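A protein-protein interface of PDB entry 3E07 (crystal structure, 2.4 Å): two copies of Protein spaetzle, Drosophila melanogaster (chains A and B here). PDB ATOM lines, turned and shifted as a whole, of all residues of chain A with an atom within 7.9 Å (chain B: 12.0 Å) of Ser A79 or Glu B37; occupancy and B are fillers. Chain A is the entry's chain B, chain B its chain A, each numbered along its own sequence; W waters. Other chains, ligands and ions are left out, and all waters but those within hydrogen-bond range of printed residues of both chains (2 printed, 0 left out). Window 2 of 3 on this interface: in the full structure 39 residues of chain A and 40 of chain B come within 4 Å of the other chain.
The backbone NH (N) of Lys B39 sits at hydrogen-bond distance from the backbone carbonyl oxygen (O) of Ala A78 (3.1 Å).
OE2 of Glu B37 lies within hydrogen-bond range of OG of Ser A79, at 2.9 Å.
OH of Tyr B38 lies within hydrogen-bond range of OD2 of Asp A87.
The backbone NH (N) of Ala B41 sits at hydrogen-bond distance from the backbone carbonyl oxygen (O) of Thr A76 (3.2 Å).
The backbone carbonyl oxygen (O) of Glu B37 lies within hydrogen-bond range of the side-chain amino group (NZ) of Lys B39.
The backbone carbonyl oxygen of Leu A77 lies within hydrogen-bond range of the backbone NH of Val A89.
The side-chain hydroxyl (OG) of Ser A79 lies within hydrogen-bond range of the side-chain amino group (NZ) of Lys A81.
The backbone carbonyl oxygen (O) of Ser A79 sits at hydrogen-bond distance from the backbone NH (N) of Asp A87 (2.6 Å).
CD1 of Tyr B38 touches O of Leu A77 (3.8 Å).
Leu A77 touches Lys B39.
Leu A77 touches Gln B40 (CD2 to CA, 3.8 Å).
Tyr B38 touches Ala A78 (CA to O, 3.5 Å).
Ser A79 touches Tyr B38.
CE1 of Tyr B38 touches CG2 of Val A89, 3.6 Å away.
Of the printed residues of chain B, Thr A76 touches Ala B41.
Printed residues of chain B within 4 Å of Leu A77: Tyr B38 (3.8 Å), Lys B39 (3.4 Å) and Gln B40 (3.8 Å).
Of chain B, only Tyr B38 (3.5 Å) and Lys B39 (3.1 Å) come within 4 Å of Ala A78.
No residue of chain B comes within 4 Å of Ile A80.
No residue of chain B comes within 4 Å of Leu A86.
Of the printed residues of chain B, Asp A87 touches Tyr B38.
No residue of chain B comes within 4 Å of Val A88.
Of the printed residues of chain B, Val A89 touches Tyr B38.
Tyr B18 touches none of the printed residues of chain A.
No residue of chain A comes within 4 Å of Asp B36.
Of chain A, only Ser A79 comes within 4 Å of Glu B37.
Printed residues of chain A within 4 Å of Lys B39: Leu A77 and Ala A78.
Of the printed residues of chain A, Gln B40 touches Leu A77 (3.8 Å).
Printed residues of chain A within 4 Å of Ala B41: Thr A76.
Ile B42 touches none of the printed residues of chain A.
The nearest residue of chain B that does not touch Ser A79 is Lys B39 (5.2 Å).
The nearest residue of chain A that does not touch Glu B37 is Lys A81 (4.2 Å).
The nearest printed residue of chain B that does not touch Val A89 is Lys B39 (7.2 Å).
Of the 10 printed residues of chain B, 5 touch a printed residue of chain A.
Hydrophobic or aromatic side chains of chain B within 4 Å of the printed part of chain A: Tyr B38 and Ala B41.
Among the printed residues, no Asp or Glu carboxylate lies within 4 Å of a Lys or Arg side-chain nitrogen of the other chain.
No position is printed for both chains.
Water W2 lies within hydrogen-bond range of the backbone carbonyl oxygen (O) of Ala B41 (2.7 Å) and the backbone NH (N) of Thr A76 (2.8 Å).
Water W1 lies within hydrogen-bond range of the side-chain hydroxyl of Ser A79 (2.8 Å), the backbone NH of Ile A80 (3.0 Å), the backbone carbonyl oxygen of Glu B37 (3.3 Å) and the side-chain amino group of Lys B39 (3.5 Å).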
ATOM      1  N   THR A  76     -14.238  23.542 -17.962  1.00  0.00           N
ATOM      2  CA  THR A  76     -14.216  22.115 -18.233  1.00  0.00           C
ATOM      3  C   THR A  76     -12.852  21.584 -18.652  1.00  0.00           C
ATOM      4  O   THR A  76     -12.232  22.086 -19.592  1.00  0.00           O
ATOM      5  CB  THR A  76     -15.275  21.742 -19.323  1.00  0.00           C
ATOM      6  OG1 THR A  76     -16.588  22.095 -18.865  1.00  0.00           O
ATOM      7  CG2 THR A  76     -15.248  20.249 -19.619  1.00  0.00           C
ATOM      8  N   LEU A  77     -12.387  20.572 -17.929  1.00  0.00           N
ATOM      9  CA  LEU A  77     -11.115  19.933 -18.231  1.00  0.00           C
ATOM     10  C   LEU A  77     -11.393  18.515 -18.701  1.00  0.00           C
ATOM     11  O   LEU A  77     -12.096  17.742 -18.038  1.00  0.00           O
ATOM     12  CB  LEU A  77     -10.208  19.904 -17.005  1.00  0.00           C
ATOM     13  CG  LEU A  77      -9.577  21.237 -16.603  1.00  0.00           C
ATOM     14  CD1 LEU A  77      -8.581  20.983 -15.481  1.00  0.00           C
ATOM     15  CD2 LEU A  77      -8.882  21.880 -17.802  1.00  0.00           C
ATOM     16  N   ALA A  78     -10.838  18.169 -19.853  1.00  0.00           N
ATOM     17  CA  ALA A  78     -11.075  16.852 -20.410  1.00  0.00           C
ATOM     18  C   ALA A  78      -9.802  16.086 -20.741  1.00  0.00           C
ATOM     19  O   ALA A  78      -8.776  16.659 -21.104  1.00  0.00           O
ATOM     20  CB  ALA A  78     -11.961  16.974 -21.652  1.00  0.00           C
ATOM     21  N   SER A  79      -9.891  14.771 -20.600  1.00  0.00           N
ATOM     22  CA  SER A  79      -8.783  13.893 -20.887  1.00  0.00           C
ATOM     23  C   SER A  79      -9.318  12.684 -21.635  1.00  0.00           C
ATOM     24  O   SER A  79     -10.359  12.124 -21.280  1.00  0.00           O
ATOM     25  CB  SER A  79      -8.108  13.443 -19.588  1.00  0.00           C
ATOM     26  OG  SER A  79      -6.980  12.631 -19.857  1.00  0.00           O
ATOM     27  N   ILE A  80      -8.609  12.306 -22.689  1.00  0.00           N
ATOM     28  CA  ILE A  80      -8.977  11.150 -23.488  1.00  0.00           C
ATOM     29  C   ILE A  80      -7.913  10.078 -23.221  1.00  0.00           C
ATOM     30  O   ILE A  80      -6.738  10.269 -23.528  1.00  0.00           O
ATOM     31  CB  ILE A  80      -9.023  11.512 -24.986  1.00  0.00           C
ATOM     32  CG1 ILE A  80     -10.070  12.610 -25.211  1.00  0.00           C
ATOM     33  CG2 ILE A  80      -9.341  10.263 -25.817  1.00  0.00           C
ATOM     34  CD1 ILE A  80     -10.086  13.172 -26.603  1.00  0.00           C
ATOM     35  N   LYS A  81      -8.331   8.962 -22.632  1.00  0.00           N
ATOM     36  CA  LYS A  81      -7.406   7.885 -22.305  1.00  0.00           C
ATOM     37  C   LYS A  81      -6.940   7.077 -23.517  1.00  0.00           C
ATOM     38  O   LYS A  81      -7.391   7.311 -24.647  1.00  0.00           O
ATOM     39  CB  LYS A  81      -8.048   6.965 -21.267  1.00  0.00           C
ATOM     40  CG  LYS A  81      -8.404   7.698 -19.987  1.00  0.00           C
ATOM     41  CD  LYS A  81      -7.173   8.390 -19.414  1.00  0.00           C
ATOM     42  CE  LYS A  81      -7.528   9.276 -18.238  1.00  0.00           C
ATOM     43  NZ  LYS A  81      -8.466  10.357 -18.644  1.00  0.00           N
ATOM     44  N   SER A  82      -6.034   6.134 -23.282  1.00  0.00           N
ATOM     45  CA  SER A  82      -5.516   5.298 -24.362  1.00  0.00           C
ATOM     46  C   SER A  82      -6.597   4.416 -24.990  1.00  0.00           C
ATOM     47  O   SER A  82      -6.462   4.003 -26.140  1.00  0.00           O
ATOM     48  CB  SER A  82      -4.374   4.418 -23.853  1.00  0.00           C
ATOM     49  OG  SER A  82      -4.845   3.509 -22.880  1.00  0.00           O
ATOM     50  N   GLY A  84      -9.548   5.477 -25.417  1.00  0.00           N
ATOM     51  CA  GLY A  84     -10.515   6.407 -25.967  1.00  0.00           C
ATOM     52  C   GLY A  84     -11.546   6.952 -25.007  1.00  0.00           C
ATOM     53  O   GLY A  84     -12.374   7.773 -25.406  1.00  0.00           O
ATOM     54  N   GLU A  85     -11.509   6.500 -23.755  1.00  0.00           N
ATOM     55  CA  GLU A  85     -12.457   6.986 -22.765  1.00  0.00           C
ATOM     56  C   GLU A  85     -12.237   8.468 -22.508  1.00  0.00           C
ATOM     57  O   GLU A  85     -11.100   8.923 -22.351  1.00  0.00           O
ATOM     58  CB  GLU A  85     -12.318   6.236 -21.446  1.00  0.00           C
ATOM     59  CG  GLU A  85     -13.025   6.959 -20.306  1.00  0.00           C
ATOM     60  CD  GLU A  85     -13.010   6.182 -19.016  1.00  0.00           C
ATOM     61  OE1 GLU A  85     -13.510   5.036 -19.025  1.00  0.00           O
ATOM     62  OE2 GLU A  85     -12.506   6.721 -18.002  1.00  0.00           O
ATOM     63  N   LEU A  86     -13.336   9.215 -22.464  1.00  0.00           N
ATOM     64  CA  LEU A  86     -13.275  10.653 -22.229  1.00  0.00           C
ATOM     65  C   LEU A  86     -13.595  10.986 -20.776  1.00  0.00           C
ATOM     66  O   LEU A  86     -14.712  10.780 -20.316  1.00  0.00           O
ATOM     67  CB  LEU A  86     -14.250  11.376 -23.159  1.00  0.00           C
ATOM     68  CG  LEU A  86     -14.449  12.880 -22.961  1.00  0.00           C
ATOM     69  CD1 LEU A  86     -13.158  13.655 -23.206  1.00  0.00           C
ATOM     70  CD2 LEU A  86     -15.519  13.329 -23.930  1.00  0.00           C
ATOM     71  N   ASP A  87     -12.600  11.494 -20.059  1.00  0.00           N
ATOM     72  CA  ASP A  87     -12.770  11.853 -18.655  1.00  0.00           C
ATOM     73  C   ASP A  87     -12.890  13.379 -18.515  1.00  0.00           C
ATOM     74  O   ASP A  87     -11.968  14.121 -18.875  1.00  0.00           O
ATOM     75  CB  ASP A  87     -11.573  11.348 -17.847  1.00  0.00           C
ATOM     76  CG  ASP A  87     -11.809  11.419 -16.354  1.00  0.00           C
ATOM     77  OD1 ASP A  87     -12.701  10.696 -15.859  1.00  0.00           O
ATOM     78  OD2 ASP A  87     -11.108  12.200 -15.678  1.00  0.00           O
ATOM     79  N   VAL A  88     -14.020  13.850 -17.997  1.00  0.00           N
ATOM     80  CA  VAL A  88     -14.221  15.291 -17.845  1.00  0.00           C
ATOM     81  C   VAL A  88     -14.354  15.764 -16.411  1.00  0.00           C
ATOM     82  O   VAL A  88     -15.069  15.170 -15.604  1.00  0.00           O
ATOM     83  CB  VAL A  88     -15.466  15.779 -18.614  1.00  0.00           C
ATOM     84  CG1 VAL A  88     -15.336  15.409 -20.080  1.00  0.00           C
ATOM     85  CG2 VAL A  88     -16.722  15.175 -18.014  1.00  0.00           C
ATOM     86  N   VAL A  89     -13.652  16.851 -16.117  1.00  0.00           N
ATOM     87  CA  VAL A  89     -13.657  17.469 -14.792  1.00  0.00           C
ATOM     88  C   VAL A  89     -14.225  18.878 -14.912  1.00  0.00           C
ATOM     89  O   VAL A  89     -13.776  19.660 -15.749  1.00  0.00           O
ATOM     90  CB  VAL A  89     -12.230  17.561 -14.230  1.00  0.00           C
ATOM     91  CG1 VAL A  89     -12.235  18.296 -12.904  1.00  0.00           C
ATOM     92  CG2 VAL A  89     -11.651  16.155 -14.085  1.00  0.00           C
ATOM     93  N   LEU B  16     -18.193  21.372 -27.096  1.00  0.00           N
ATOM     94  CA  LEU B  16     -16.883  21.549 -26.470  1.00  0.00           C
ATOM     95  C   LEU B  16     -15.816  21.809 -27.520  1.00  0.00           C
ATOM     96  O   LEU B  16     -15.704  21.080 -28.493  1.00  0.00           O
ATOM     97  CB  LEU B  16     -16.499  20.307 -25.681  1.00  0.00           C
ATOM     98  CG  LEU B  16     -16.725  20.350 -24.175  1.00  0.00           C
ATOM     99  CD1 LEU B  16     -16.215  19.044 -23.579  1.00  0.00           C
ATOM    100  CD2 LEU B  16     -15.986  21.544 -23.570  1.00  0.00           C
ATOM    101  N   VAL B  17     -15.016  22.842 -27.314  1.00  0.00           N
ATOM    102  CA  VAL B  17     -13.989  23.182 -28.280  1.00  0.00           C
ATOM    103  C   VAL B  17     -12.630  23.330 -27.617  1.00  0.00           C
ATOM    104  O   VAL B  17     -12.530  23.473 -26.395  1.00  0.00           O
ATOM    105  CB  VAL B  17     -14.364  24.486 -29.020  1.00  0.00           C
ATOM    106  CG1 VAL B  17     -13.302  24.845 -30.049  1.00  0.00           C
ATOM    107  CG2 VAL B  17     -15.699  24.306 -29.706  1.00  0.00           C
ATOM    108  N   TYR B  18     -11.587  23.293 -28.437  1.00  0.00           N
ATOM    109  CA  TYR B  18     -10.220  23.415 -27.950  1.00  0.00           C
ATOM    110  C   TYR B  18      -9.483  24.621 -28.527  1.00  0.00           C
ATOM    111  O   TYR B  18      -9.507  24.869 -29.737  1.00  0.00           O
ATOM    112  CB  TYR B  18      -9.432  22.156 -28.294  1.00  0.00           C
ATOM    113  CG  TYR B  18      -9.808  20.934 -27.510  1.00  0.00           C
ATOM    114  CD1 TYR B  18      -9.016  20.496 -26.453  1.00  0.00           C
ATOM    115  CD2 TYR B  18     -10.930  20.178 -27.852  1.00  0.00           C
ATOM    116  CE1 TYR B  18      -9.321  19.326 -25.758  1.00  0.00           C
ATOM    117  CE2 TYR B  18     -11.248  19.008 -27.163  1.00  0.00           C
ATOM    118  CZ  TYR B  18     -10.433  18.584 -26.120  1.00  0.00           C
ATOM    119  OH  TYR B  18     -10.694  17.396 -25.469  1.00  0.00           O
ATOM    120  N   ASP B  36      -3.722  17.517 -14.727  1.00  0.00           N
ATOM    121  CA  ASP B  36      -2.356  17.245 -15.165  1.00  0.00           C
ATOM    122  C   ASP B  36      -2.278  17.136 -16.687  1.00  0.00           C
ATOM    123  O   ASP B  36      -1.747  18.029 -17.345  1.00  0.00           O
ATOM    124  CB  ASP B  36      -1.850  15.958 -14.511  1.00  0.00           C
ATOM    125  CG  ASP B  36      -2.677  14.745 -14.891  1.00  0.00           C
ATOM    126  OD1 ASP B  36      -2.214  13.957 -15.746  1.00  0.00           O
ATOM    127  OD2 ASP B  36      -3.792  14.586 -14.342  1.00  0.00           O
ATOM    128  N   GLU B  37      -2.797  16.039 -17.242  1.00  0.00           N
ATOM    129  CA  GLU B  37      -2.797  15.843 -18.690  1.00  0.00           C
ATOM    130  C   GLU B  37      -4.172  16.180 -19.239  1.00  0.00           C
ATOM    131  O   GLU B  37      -4.572  15.708 -20.306  1.00  0.00           O
ATOM    132  CB  GLU B  37      -2.431  14.404 -19.076  1.00  0.00           C
ATOM    133  CG  GLU B  37      -3.465  13.346 -18.721  1.00  0.00           C
ATOM    134  CD  GLU B  37      -3.309  12.088 -19.567  1.00  0.00           C
ATOM    135  OE1 GLU B  37      -2.153  11.686 -19.827  1.00  0.00           O
ATOM    136  OE2 GLU B  37      -4.337  11.498 -19.972  1.00  0.00           O
ATOM    137  N   TYR B  38      -4.904  16.987 -18.481  1.00  0.00           N
ATOM    138  CA  TYR B  38      -6.224  17.432 -18.893  1.00  0.00           C
ATOM    139  C   TYR B  38      -6.041  18.748 -19.644  1.00  0.00           C
ATOM    140  O   TYR B  38      -5.343  19.644 -19.176  1.00  0.00           O
ATOM    141  CB  TYR B  38      -7.121  17.637 -17.669  1.00  0.00           C
ATOM    142  CG  TYR B  38      -7.546  16.348 -17.010  1.00  0.00           C
ATOM    143  CD1 TYR B  38      -8.889  15.976 -16.974  1.00  0.00           C
ATOM    144  CD2 TYR B  38      -6.603  15.484 -16.447  1.00  0.00           C
ATOM    145  CE1 TYR B  38      -9.290  14.770 -16.396  1.00  0.00           C
ATOM    146  CE2 TYR B  38      -6.991  14.277 -15.867  1.00  0.00           C
ATOM    147  CZ  TYR B  38      -8.337  13.924 -15.849  1.00  0.00           C
ATOM    148  OH  TYR B  38      -8.727  12.722 -15.304  1.00  0.00           O
ATOM    149  N   LYS B  39      -6.638  18.847 -20.824  1.00  0.00           N
ATOM    150  CA  LYS B  39      -6.526  20.058 -21.612  1.00  0.00           C
ATOM    151  C   LYS B  39      -7.750  20.905 -21.332  1.00  0.00           C
ATOM    152  O   LYS B  39      -8.779  20.401 -20.890  1.00  0.00           O
ATOM    153  CB  LYS B  39      -6.467  19.736 -23.111  1.00  0.00           C
ATOM    154  CG  LYS B  39      -5.587  18.554 -23.482  1.00  0.00           C
ATOM    155  CD  LYS B  39      -4.166  18.693 -22.955  1.00  0.00           C
ATOM    156  CE  LYS B  39      -3.297  17.540 -23.445  1.00  0.00           C
ATOM    157  NZ  LYS B  39      -3.914  16.207 -23.160  1.00  0.00           N
ATOM    158  N   GLN B  40      -7.629  22.199 -21.589  1.00  0.00           N
ATOM    159  CA  GLN B  40      -8.737  23.109 -21.383  1.00  0.00           C
ATOM    160  C   GLN B  40      -9.632  23.030 -22.606  1.00  0.00           C
ATOM    161  O   GLN B  40      -9.176  23.169 -23.744  1.00  0.00           O
ATOM    162  CB  GLN B  40      -8.227  24.537 -21.209  1.00  0.00           C
ATOM    163  CG  GLN B  40      -9.303  25.532 -20.832  1.00  0.00           C
ATOM    164  CD  GLN B  40      -9.165  26.843 -21.582  1.00  0.00           C
ATOM    165  OE1 GLN B  40      -9.559  27.899 -21.086  1.00  0.00           O
ATOM    166  NE2 GLN B  40      -8.615  26.778 -22.794  1.00  0.00           N
ATOM    167  N   ALA B  41     -10.909  22.776 -22.369  1.00  0.00           N
ATOM    168  CA  ALA B  41     -11.860  22.700 -23.455  1.00  0.00           C
ATOM    169  C   ALA B  41     -12.870  23.796 -23.170  1.00  0.00           C
ATOM    170  O   ALA B  41     -13.315  23.966 -22.036  1.00  0.00           O
ATOM    171  CB  ALA B  41     -12.523  21.331 -23.486  1.00  0.00           C
ATOM    172  N   ILE B  42     -13.227  24.535 -24.209  1.00  0.00           N
ATOM    173  CA  ILE B  42     -14.145  25.651 -24.061  1.00  0.00           C
ATOM    174  C   ILE B  42     -15.572  25.334 -24.482  1.00  0.00           C
ATOM    175  O   ILE B  42     -15.807  24.892 -25.606  1.00  0.00           O
ATOM    176  CB  ILE B  42     -13.628  26.858 -24.885  1.00  0.00           C
ATOM    177  CG1 ILE B  42     -12.256  27.280 -24.349  1.00  0.00           C
ATOM    178  CG2 ILE B  42     -14.625  28.011 -24.832  1.00  0.00           C
ATOM    179  CD1 ILE B  42     -11.558  28.324 -25.186  1.00  0.00           C
HETATM  180  O   HOH W   1      -5.791  13.402 -22.294  1.00  0.00           O
HETATM  181  O   HOH W   2     -13.527  25.482 -19.850  1.00  0.00           O
